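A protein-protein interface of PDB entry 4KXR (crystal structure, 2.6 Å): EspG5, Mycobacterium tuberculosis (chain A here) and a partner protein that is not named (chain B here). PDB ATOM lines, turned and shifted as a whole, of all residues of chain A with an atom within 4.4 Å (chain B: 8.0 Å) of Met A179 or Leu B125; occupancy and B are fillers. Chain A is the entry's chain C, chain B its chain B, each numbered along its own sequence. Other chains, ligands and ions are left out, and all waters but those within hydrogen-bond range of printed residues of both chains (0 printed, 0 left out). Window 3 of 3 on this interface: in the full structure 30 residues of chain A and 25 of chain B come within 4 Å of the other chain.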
ATOM      1  N   VAL A 174     -16.257  -1.641 -23.567  1.00  0.00           N
ATOM      2  CA  VAL A 174     -16.554  -1.254 -24.944  1.00  0.00           C
ATOM      3  C   VAL A 174     -18.051  -1.050 -25.152  1.00  0.00           C
ATOM      4  O   VAL A 174     -18.868  -1.677 -24.456  1.00  0.00           O
ATOM      5  CB  VAL A 174     -16.015  -2.284 -25.959  1.00  0.00           C
ATOM      6  CG1 VAL A 174     -14.517  -2.465 -25.764  1.00  0.00           C
ATOM      7  CG2 VAL A 174     -16.718  -3.623 -25.827  1.00  0.00           C
ATOM      8  N   PRO A 175     -18.424  -0.174 -26.107  1.00  0.00           N
ATOM      9  CA  PRO A 175     -19.845   0.037 -26.382  1.00  0.00           C
ATOM     10  C   PRO A 175     -20.519  -1.231 -26.891  1.00  0.00           C
ATOM     11  O   PRO A 175     -20.007  -1.891 -27.800  1.00  0.00           O
ATOM     12  CB  PRO A 175     -19.855   1.124 -27.459  1.00  0.00           C
ATOM     13  CG  PRO A 175     -18.528   1.773 -27.372  1.00  0.00           C
ATOM     14  CD  PRO A 175     -17.582   0.687 -26.948  1.00  0.00           C
ATOM     15  N   MET A 176     -21.669  -1.543 -26.293  1.00  0.00           N
ATOM     16  CA  MET A 176     -22.361  -2.795 -26.521  1.00  0.00           C
ATOM     17  C   MET A 176     -22.781  -2.943 -27.978  1.00  0.00           C
ATOM     18  O   MET A 176     -22.543  -3.980 -28.577  1.00  0.00           O
ATOM     19  CB  MET A 176     -23.583  -2.889 -25.600  1.00  0.00           C
ATOM     20  CG  MET A 176     -24.427  -4.143 -25.783  1.00  0.00           C
ATOM     21  SD  MET A 176     -23.465  -5.652 -25.615  1.00  0.00           S
ATOM     22  CE  MET A 176     -23.721  -5.878 -23.874  1.00  0.00           C
ATOM     23  N   GLU A 177     -23.401  -1.912 -28.534  1.00  0.00           N
ATOM     24  CA  GLU A 177     -23.924  -1.981 -29.884  1.00  0.00           C
ATOM     25  C   GLU A 177     -22.774  -2.265 -30.862  1.00  0.00           C
ATOM     26  O   GLU A 177     -22.874  -3.170 -31.671  1.00  0.00           O
ATOM     27  CB  GLU A 177     -24.669  -0.681 -30.241  1.00  0.00           C
ATOM     28  CG  GLU A 177     -25.529  -0.739 -31.509  1.00  0.00           C
ATOM     29  CD  GLU A 177     -25.952   0.650 -32.047  1.00  0.00           C
ATOM     30  OE1 GLU A 177     -25.402   1.697 -31.606  1.00  0.00           O
ATOM     31  OE2 GLU A 177     -26.838   0.709 -32.938  1.00  0.00           O
ATOM     32  N   GLU A 178     -21.680  -1.513 -30.765  1.00  0.00           N
ATOM     33  CA  GLU A 178     -20.548  -1.634 -31.689  1.00  0.00           C
ATOM     34  C   GLU A 178     -19.854  -3.001 -31.580  1.00  0.00           C
ATOM     35  O   GLU A 178     -19.470  -3.608 -32.587  1.00  0.00           O
ATOM     36  CB  GLU A 178     -19.539  -0.505 -31.445  1.00  0.00           C
ATOM     37  CG  GLU A 178     -19.903   0.856 -32.062  1.00  0.00           C
ATOM     38  CD  GLU A 178     -21.037   1.633 -31.352  1.00  0.00           C
ATOM     39  OE1 GLU A 178     -21.548   1.174 -30.298  1.00  0.00           O
ATOM     40  OE2 GLU A 178     -21.429   2.726 -31.863  1.00  0.00           O
ATOM     41  N   MET A 179     -19.710  -3.488 -30.354  1.00  0.00           N
ATOM     42  CA  MET A 179     -19.126  -4.797 -30.103  1.00  0.00           C
ATOM     43  C   MET A 179     -19.940  -5.961 -30.681  1.00  0.00           C
ATOM     44  O   MET A 179     -19.357  -6.952 -31.102  1.00  0.00           O
ATOM     45  CB  MET A 179     -18.951  -4.978 -28.602  1.00  0.00           C
ATOM     46  CG  MET A 179     -18.242  -6.245 -28.175  1.00  0.00           C
ATOM     47  SD  MET A 179     -16.560  -6.399 -28.777  1.00  0.00           S
ATOM     48  CE  MET A 179     -16.169  -8.080 -28.296  1.00  0.00           C
ATOM     49  N   LEU A 180     -21.271  -5.844 -30.706  1.00  0.00           N
ATOM     50  CA  LEU A 180     -22.150  -6.884 -31.274  1.00  0.00           C
ATOM     51  C   LEU A 180     -22.052  -6.927 -32.765  1.00  0.00           C
ATOM     52  O   LEU A 180     -22.006  -8.008 -33.352  1.00  0.00           O
ATOM     53  CB  LEU A 180     -23.627  -6.626 -30.959  1.00  0.00           C
ATOM     54  CG  LEU A 180     -24.116  -6.867 -29.541  1.00  0.00           C
ATOM     55  CD1 LEU A 180     -25.500  -6.239 -29.404  1.00  0.00           C
ATOM     56  CD2 LEU A 180     -24.146  -8.357 -29.215  1.00  0.00           C
ATOM     57  N   GLU A 181     -22.099  -5.745 -33.372  1.00  0.00           N
ATOM     58  CA  GLU A 181     -21.938  -5.601 -34.811  1.00  0.00           C
ATOM     59  C   GLU A 181     -20.581  -6.191 -35.221  1.00  0.00           C
ATOM     60  O   GLU A 181     -20.513  -6.984 -36.150  1.00  0.00           O
ATOM     61  CB  GLU A 181     -22.067  -4.121 -35.217  1.00  0.00           C
ATOM     62  CG  GLU A 181     -22.029  -3.829 -36.714  1.00  0.00           C
ATOM     63  CD  GLU A 181     -23.161  -4.506 -37.491  1.00  0.00           C
ATOM     64  OE1 GLU A 181     -23.153  -5.758 -37.600  1.00  0.00           O
ATOM     65  OE2 GLU A 181     -24.057  -3.791 -38.014  1.00  0.00           O
ATOM     66  N   ALA A 182     -19.520  -5.845 -34.489  1.00  0.00           N
ATOM     67  CA  ALA A 182     -18.170  -6.332 -34.800  1.00  0.00           C
ATOM     68  C   ALA A 182     -17.997  -7.824 -34.525  1.00  0.00           C
ATOM     69  O   ALA A 182     -17.376  -8.538 -35.316  1.00  0.00           O
ATOM     70  CB  ALA A 182     -17.119  -5.541 -34.041  1.00  0.00           C
ATOM     71  N   THR A 183     -18.542  -8.294 -33.408  1.00  0.00           N
ATOM     72  CA  THR A 183     -18.536  -9.713 -33.128  1.00  0.00           C
ATOM     73  C   THR A 183     -19.351 -10.524 -34.144  1.00  0.00           C
ATOM     74  O   THR A 183     -19.045 -11.685 -34.384  1.00  0.00           O
ATOM     75  CB  THR A 183     -19.018 -10.001 -31.713  1.00  0.00           C
ATOM     76  OG1 THR A 183     -18.157  -9.346 -30.771  1.00  0.00           O
ATOM     77  CG2 THR A 183     -18.976 -11.480 -31.435  1.00  0.00           C
ATOM     78  N   LEU A 199     -12.138  -5.398 -33.950  1.00  0.00           N
ATOM     79  CA  LEU A 199     -12.095  -5.388 -32.476  1.00  0.00           C
ATOM     80  C   LEU A 199     -10.827  -4.684 -31.979  1.00  0.00           C
ATOM     81  O   LEU A 199     -10.850  -3.981 -30.981  1.00  0.00           O
ATOM     82  CB  LEU A 199     -12.190  -6.805 -31.896  1.00  0.00           C
ATOM     83  CG  LEU A 199     -13.584  -7.462 -31.954  1.00  0.00           C
ATOM     84  CD1 LEU A 199     -14.046  -7.782 -33.369  1.00  0.00           C
ATOM     85  CD2 LEU A 199     -13.600  -8.733 -31.113  1.00  0.00           C
ATOM     86  N   MET A 202     -11.328  -0.800 -31.978  1.00  0.00           N
ATOM     87  CA  MET A 202     -12.126  -0.282 -30.863  1.00  0.00           C
ATOM     88  C   MET A 202     -11.262  -0.153 -29.606  1.00  0.00           C
ATOM     89  O   MET A 202     -11.753   0.231 -28.539  1.00  0.00           O
ATOM     90  CB  MET A 202     -13.312  -1.218 -30.538  1.00  0.00           C
ATOM     91  CG  MET A 202     -14.298  -1.516 -31.669  1.00  0.00           C
ATOM     92  SD  MET A 202     -15.561  -2.743 -31.201  1.00  0.00           S
ATOM     93  CE  MET A 202     -16.425  -1.838 -29.925  1.00  0.00           C
ATOM     94  N   ILE A 204      -9.519  -2.759 -28.141  1.00  0.00           N
ATOM     95  CA  ILE A 204      -9.402  -3.976 -27.364  1.00  0.00           C
ATOM     96  C   ILE A 204      -7.994  -4.530 -27.607  1.00  0.00           C
ATOM     97  O   ILE A 204      -7.549  -4.585 -28.745  1.00  0.00           O
ATOM     98  CB  ILE A 204     -10.477  -5.006 -27.776  1.00  0.00           C
ATOM     99  CG1 ILE A 204     -11.883  -4.401 -27.658  1.00  0.00           C
ATOM    100  CG2 ILE A 204     -10.376  -6.258 -26.919  1.00  0.00           C
ATOM    101  CD1 ILE A 204     -12.987  -5.280 -28.212  1.00  0.00           C
ATOM    102  N   LEU A 212     -10.352 -14.078 -26.324  1.00  0.00           N
ATOM    103  CA  LEU A 212     -11.777 -14.055 -26.617  1.00  0.00           C
ATOM    104  C   LEU A 212     -12.088 -14.883 -27.877  1.00  0.00           C
ATOM    105  O   LEU A 212     -13.036 -15.660 -27.896  1.00  0.00           O
ATOM    106  CB  LEU A 212     -12.252 -12.615 -26.762  1.00  0.00           C
ATOM    107  CG  LEU A 212     -13.720 -12.429 -27.130  1.00  0.00           C
ATOM    108  CD1 LEU A 212     -14.659 -13.003 -26.064  1.00  0.00           C
ATOM    109  CD2 LEU A 212     -14.006 -10.955 -27.350  1.00  0.00           C
ATOM    110  N   SER A 243     -21.591 -13.708 -18.530  1.00  0.00           N
ATOM    111  CA  SER A 243     -21.204 -14.852 -19.344  1.00  0.00           C
ATOM    112  C   SER A 243     -19.751 -15.203 -19.107  1.00  0.00           C
ATOM    113  O   SER A 243     -18.904 -14.323 -19.145  1.00  0.00           O
ATOM    114  CB  SER A 243     -21.388 -14.538 -20.804  1.00  0.00           C
ATOM    115  OG  SER A 243     -20.876 -15.606 -21.556  1.00  0.00           O
ATOM    116  N   LEU A 254     -17.698 -11.884 -19.580  1.00  0.00           N
ATOM    117  CA  LEU A 254     -18.403 -10.837 -20.309  1.00  0.00           C
ATOM    118  C   LEU A 254     -19.644 -10.454 -19.532  1.00  0.00           C
ATOM    119  O   LEU A 254     -20.396 -11.330 -19.103  1.00  0.00           O
ATOM    120  CB  LEU A 254     -18.815 -11.356 -21.679  1.00  0.00           C
ATOM    121  CG  LEU A 254     -17.661 -11.794 -22.568  1.00  0.00           C
ATOM    122  CD1 LEU A 254     -18.159 -12.656 -23.718  1.00  0.00           C
ATOM    123  CD2 LEU A 254     -16.916 -10.570 -23.080  1.00  0.00           C
ATOM    124  N   LEU A 268     -20.272  -3.174 -22.557  1.00  0.00           N
ATOM    125  CA  LEU A 268     -19.886  -4.528 -22.197  1.00  0.00           C
ATOM    126  C   LEU A 268     -18.540  -4.453 -21.497  1.00  0.00           C
ATOM    127  O   LEU A 268     -17.621  -3.780 -21.975  1.00  0.00           O
ATOM    128  CB  LEU A 268     -19.771  -5.392 -23.459  1.00  0.00           C
ATOM    129  CG  LEU A 268     -19.578  -6.909 -23.357  1.00  0.00           C
ATOM    130  CD1 LEU A 268     -20.772  -7.607 -22.727  1.00  0.00           C
ATOM    131  CD2 LEU A 268     -19.324  -7.518 -24.734  1.00  0.00           C
ATOM    132  N   ILE A 270     -15.329  -6.607 -20.656  1.00  0.00           N
ATOM    133  CA  ILE A 270     -14.607  -7.812 -21.058  1.00  0.00           C
ATOM    134  C   ILE A 270     -13.490  -7.927 -20.037  1.00  0.00           C
ATOM    135  O   ILE A 270     -12.725  -6.988 -19.856  1.00  0.00           O
ATOM    136  CB  ILE A 270     -14.018  -7.697 -22.474  1.00  0.00           C
ATOM    137  CG1 ILE A 270     -15.025  -7.067 -23.440  1.00  0.00           C
ATOM    138  CG2 ILE A 270     -13.583  -9.065 -22.981  1.00  0.00           C
ATOM    139  CD1 ILE A 270     -14.568  -7.052 -24.889  1.00  0.00           C
ATOM    140  N   LEU B 119     -32.169 -14.828 -31.841  1.00  0.00           N
ATOM    141  CA  LEU B 119     -31.419 -14.410 -30.667  1.00  0.00           C
ATOM    142  C   LEU B 119     -30.240 -15.351 -30.414  1.00  0.00           C
ATOM    143  O   LEU B 119     -29.140 -14.895 -30.083  1.00  0.00           O
ATOM    144  CB  LEU B 119     -32.308 -14.303 -29.427  1.00  0.00           C
ATOM    145  CG  LEU B 119     -33.401 -13.226 -29.448  1.00  0.00           C
ATOM    146  CD1 LEU B 119     -34.014 -13.103 -28.059  1.00  0.00           C
ATOM    147  CD2 LEU B 119     -32.930 -11.852 -29.915  1.00  0.00           C
ATOM    148  N   ILE B 120     -30.465 -16.651 -30.593  1.00  0.00           N
ATOM    149  CA  ILE B 120     -29.417 -17.650 -30.366  1.00  0.00           C
ATOM    150  C   ILE B 120     -28.312 -17.516 -31.393  1.00  0.00           C
ATOM    151  O   ILE B 120     -27.134 -17.542 -31.056  1.00  0.00           O
ATOM    152  CB  ILE B 120     -29.993 -19.083 -30.387  1.00  0.00           C
ATOM    153  CG1 ILE B 120     -30.659 -19.350 -29.049  1.00  0.00           C
ATOM    154  CG2 ILE B 120     -28.896 -20.117 -30.599  1.00  0.00           C
ATOM    155  CD1 ILE B 120     -31.504 -20.590 -29.008  1.00  0.00           C
ATOM    156  N   ASN B 122     -27.331 -14.968 -32.608  1.00  0.00           N
ATOM    157  CA  ASN B 122     -26.622 -13.721 -32.266  1.00  0.00           C
ATOM    158  C   ASN B 122     -26.145 -13.648 -30.805  1.00  0.00           C
ATOM    159  O   ASN B 122     -25.853 -12.553 -30.303  1.00  0.00           O
ATOM    160  CB  ASN B 122     -27.537 -12.506 -32.526  1.00  0.00           C
ATOM    161  CG  ASN B 122     -27.870 -12.321 -34.000  1.00  0.00           C
ATOM    162  OD1 ASN B 122     -26.986 -12.136 -34.812  1.00  0.00           O
ATOM    163  ND2 ASN B 122     -29.140 -12.368 -34.342  1.00  0.00           N
ATOM    164  N   ASN B 123     -26.048 -14.798 -30.128  1.00  0.00           N
ATOM    165  CA  ASN B 123     -25.781 -14.811 -28.685  1.00  0.00           C
ATOM    166  C   ASN B 123     -24.357 -15.194 -28.282  1.00  0.00           C
ATOM    167  O   ASN B 123     -24.140 -15.733 -27.190  1.00  0.00           O
ATOM    168  CB  ASN B 123     -26.787 -15.714 -27.970  1.00  0.00           C
ATOM    169  CG  ASN B 123     -26.944 -15.360 -26.498  1.00  0.00           C
ATOM    170  OD1 ASN B 123     -26.721 -14.208 -26.092  1.00  0.00           O
ATOM    171  ND2 ASN B 123     -27.325 -16.352 -25.687  1.00  0.00           N
ATOM    172  N   ALA B 124     -23.384 -14.880 -29.141  1.00  0.00           N
ATOM    173  CA  ALA B 124     -21.981 -15.198 -28.889  1.00  0.00           C
ATOM    174  C   ALA B 124     -21.536 -14.631 -27.554  1.00  0.00           C
ATOM    175  O   ALA B 124     -20.866 -15.299 -26.770  1.00  0.00           O
ATOM    176  CB  ALA B 124     -21.108 -14.647 -30.001  1.00  0.00           C
ATOM    177  N   LEU B 125     -21.927 -13.398 -27.291  1.00  0.00           N
ATOM    178  CA  LEU B 125     -21.517 -12.720 -26.070  1.00  0.00           C
ATOM    179  C   LEU B 125     -22.501 -12.952 -24.912  1.00  0.00           C
ATOM    180  O   LEU B 125     -22.315 -12.413 -23.800  1.00  0.00           O
ATOM    181  CB  LEU B 125     -21.336 -11.218 -26.344  1.00  0.00           C
ATOM    182  CG  LEU B 125     -20.395 -10.952 -27.518  1.00  0.00           C
ATOM    183  CD1 LEU B 125     -20.428  -9.502 -27.969  1.00  0.00           C
ATOM    184  CD2 LEU B 125     -18.987 -11.374 -27.151  1.00  0.00           C
ATOM    185  N   GLY B 126     -23.540 -13.743 -25.161  1.00  0.00           N
ATOM    186  CA  GLY B 126     -24.447 -14.157 -24.094  1.00  0.00           C
ATOM    187  C   GLY B 126     -25.487 -13.149 -23.593  1.00  0.00           C
ATOM    188  O   GLY B 126     -26.239 -13.466 -22.685  1.00  0.00           O
ATOM    189  N   GLN B 127     -25.576 -11.970 -24.202  1.00  0.00           N
ATOM    190  CA  GLN B 127     -26.407 -10.889 -23.647  1.00  0.00           C
ATOM    191  C   GLN B 127     -27.889 -10.954 -24.031  1.00  0.00           C
ATOM    192  O   GLN B 127     -28.673 -10.128 -23.593  1.00  0.00           O
ATOM    193  CB  GLN B 127     -25.823  -9.512 -24.009  1.00  0.00           C
ATOM    194  CG  GLN B 127     -24.392  -9.316 -23.533  1.00  0.00           C
ATOM    195  CD  GLN B 127     -24.227  -9.550 -22.033  1.00  0.00           C
ATOM    196  OE1 GLN B 127     -24.758  -8.807 -21.204  1.00  0.00           O
ATOM    197  NE2 GLN B 127     -23.475 -10.576 -21.682  1.00  0.00           N
ATOM    198  N   PHE B 128     -28.273 -11.950 -24.817  1.00  0.00           N
ATOM    199  CA  PHE B 128     -29.673 -12.169 -25.163  1.00  0.00           C
ATOM    200  C   PHE B 128     -30.274 -13.303 -24.373  1.00  0.00           C
ATOM    201  O   PHE B 128     -31.437 -13.623 -24.555  1.00  0.00           O
ATOM    202  CB  PHE B 128     -29.814 -12.465 -26.656  1.00  0.00           C
ATOM    203  CG  PHE B 128     -29.451 -11.310 -27.525  1.00  0.00           C
ATOM    204  CD1 PHE B 128     -30.148 -10.109 -27.427  1.00  0.00           C
ATOM    205  CD2 PHE B 128     -28.414 -11.409 -28.441  1.00  0.00           C
ATOM    206  CE1 PHE B 128     -29.811  -9.023 -28.224  1.00  0.00           C
ATOM    207  CE2 PHE B 128     -28.078 -10.331 -29.245  1.00  0.00           C
ATOM    208  CZ  PHE B 128     -28.780  -9.138 -29.136  1.00  0.00           C
ATOM    209  N   THR B 129     -29.493 -13.889 -23.471  1.00  0.00           N
ATOM    210  CA  THR B 129     -29.876 -15.140 -22.813  1.00  0.00           C
ATOM    211  C   THR B 129     -31.149 -15.005 -21.973  1.00  0.00           C
ATOM    212  O   THR B 129     -31.942 -15.945 -21.900  1.00  0.00           O
ATOM    213  CB  THR B 129     -28.726 -15.682 -21.951  1.00  0.00           C
ATOM    214  OG1 THR B 129     -27.501 -15.606 -22.701  1.00  0.00           O
ATOM    215  CG2 THR B 129     -28.980 -17.114 -21.544  1.00  0.00           C
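Met A176 touches Gln B127. Met A179 touches Leu B125. Leu B125 touches Thr A183 (CD1 to OG1, 3.6 Å). O of Leu B125 touches CB of Ser A243, 3.8 Å away. Leu A254 touches Leu B125 (CD1 to CD2, 3.8 Å). Leu A268 touches Leu B125 (CD2 to CD1, 3.95 Å).
Of the 10 printed residues of chain B, 2 touch a printed residue of chain A. Hydrophobic or aromatic side chains of chain A that line the printed part of chain B: Met A176, Met A179, Leu A254 and Leu A268.
Met A179 touches just one residue of chain B: Leu B125 (3.9 Å). Of the printed residues of chain A, Gln B127 touches Met A176. Of the printed residues of chain B, Met A176 touches Gln B127. Of the printed residues of chain B, Leu A254 touches Leu B125. Printed residues of chain B within 4 Å of Thr A183: Leu B125 (3.6 Å). Leu A180 touches none of the printed residues of chain B. Ile A204 touches none of the printed residues of chain B. The nearest printed residue of chain A that does not touch Gln B127 is Leu A268 (4.02 Å).
The backbone NH of Gln B127 lies within hydrogen-bond range of the side-chain amide oxygen of Asn B123 (3.1 Å). NE2 of Gln B127 lies within hydrogen-bond range of O of Leu B125 (3.0 Å). The backbone carbonyl oxygen of Val A174 lies within hydrogen-bond range of the backbone NH of Leu A268 (2.8 Å). OG1 of Thr A183 is in hydrogen-bond range of O of Met A179. The backbone NH of Ser A243 lies within hydrogen-bond range of the backbone carbonyl oxygen of Leu A254 (2.7 Å).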
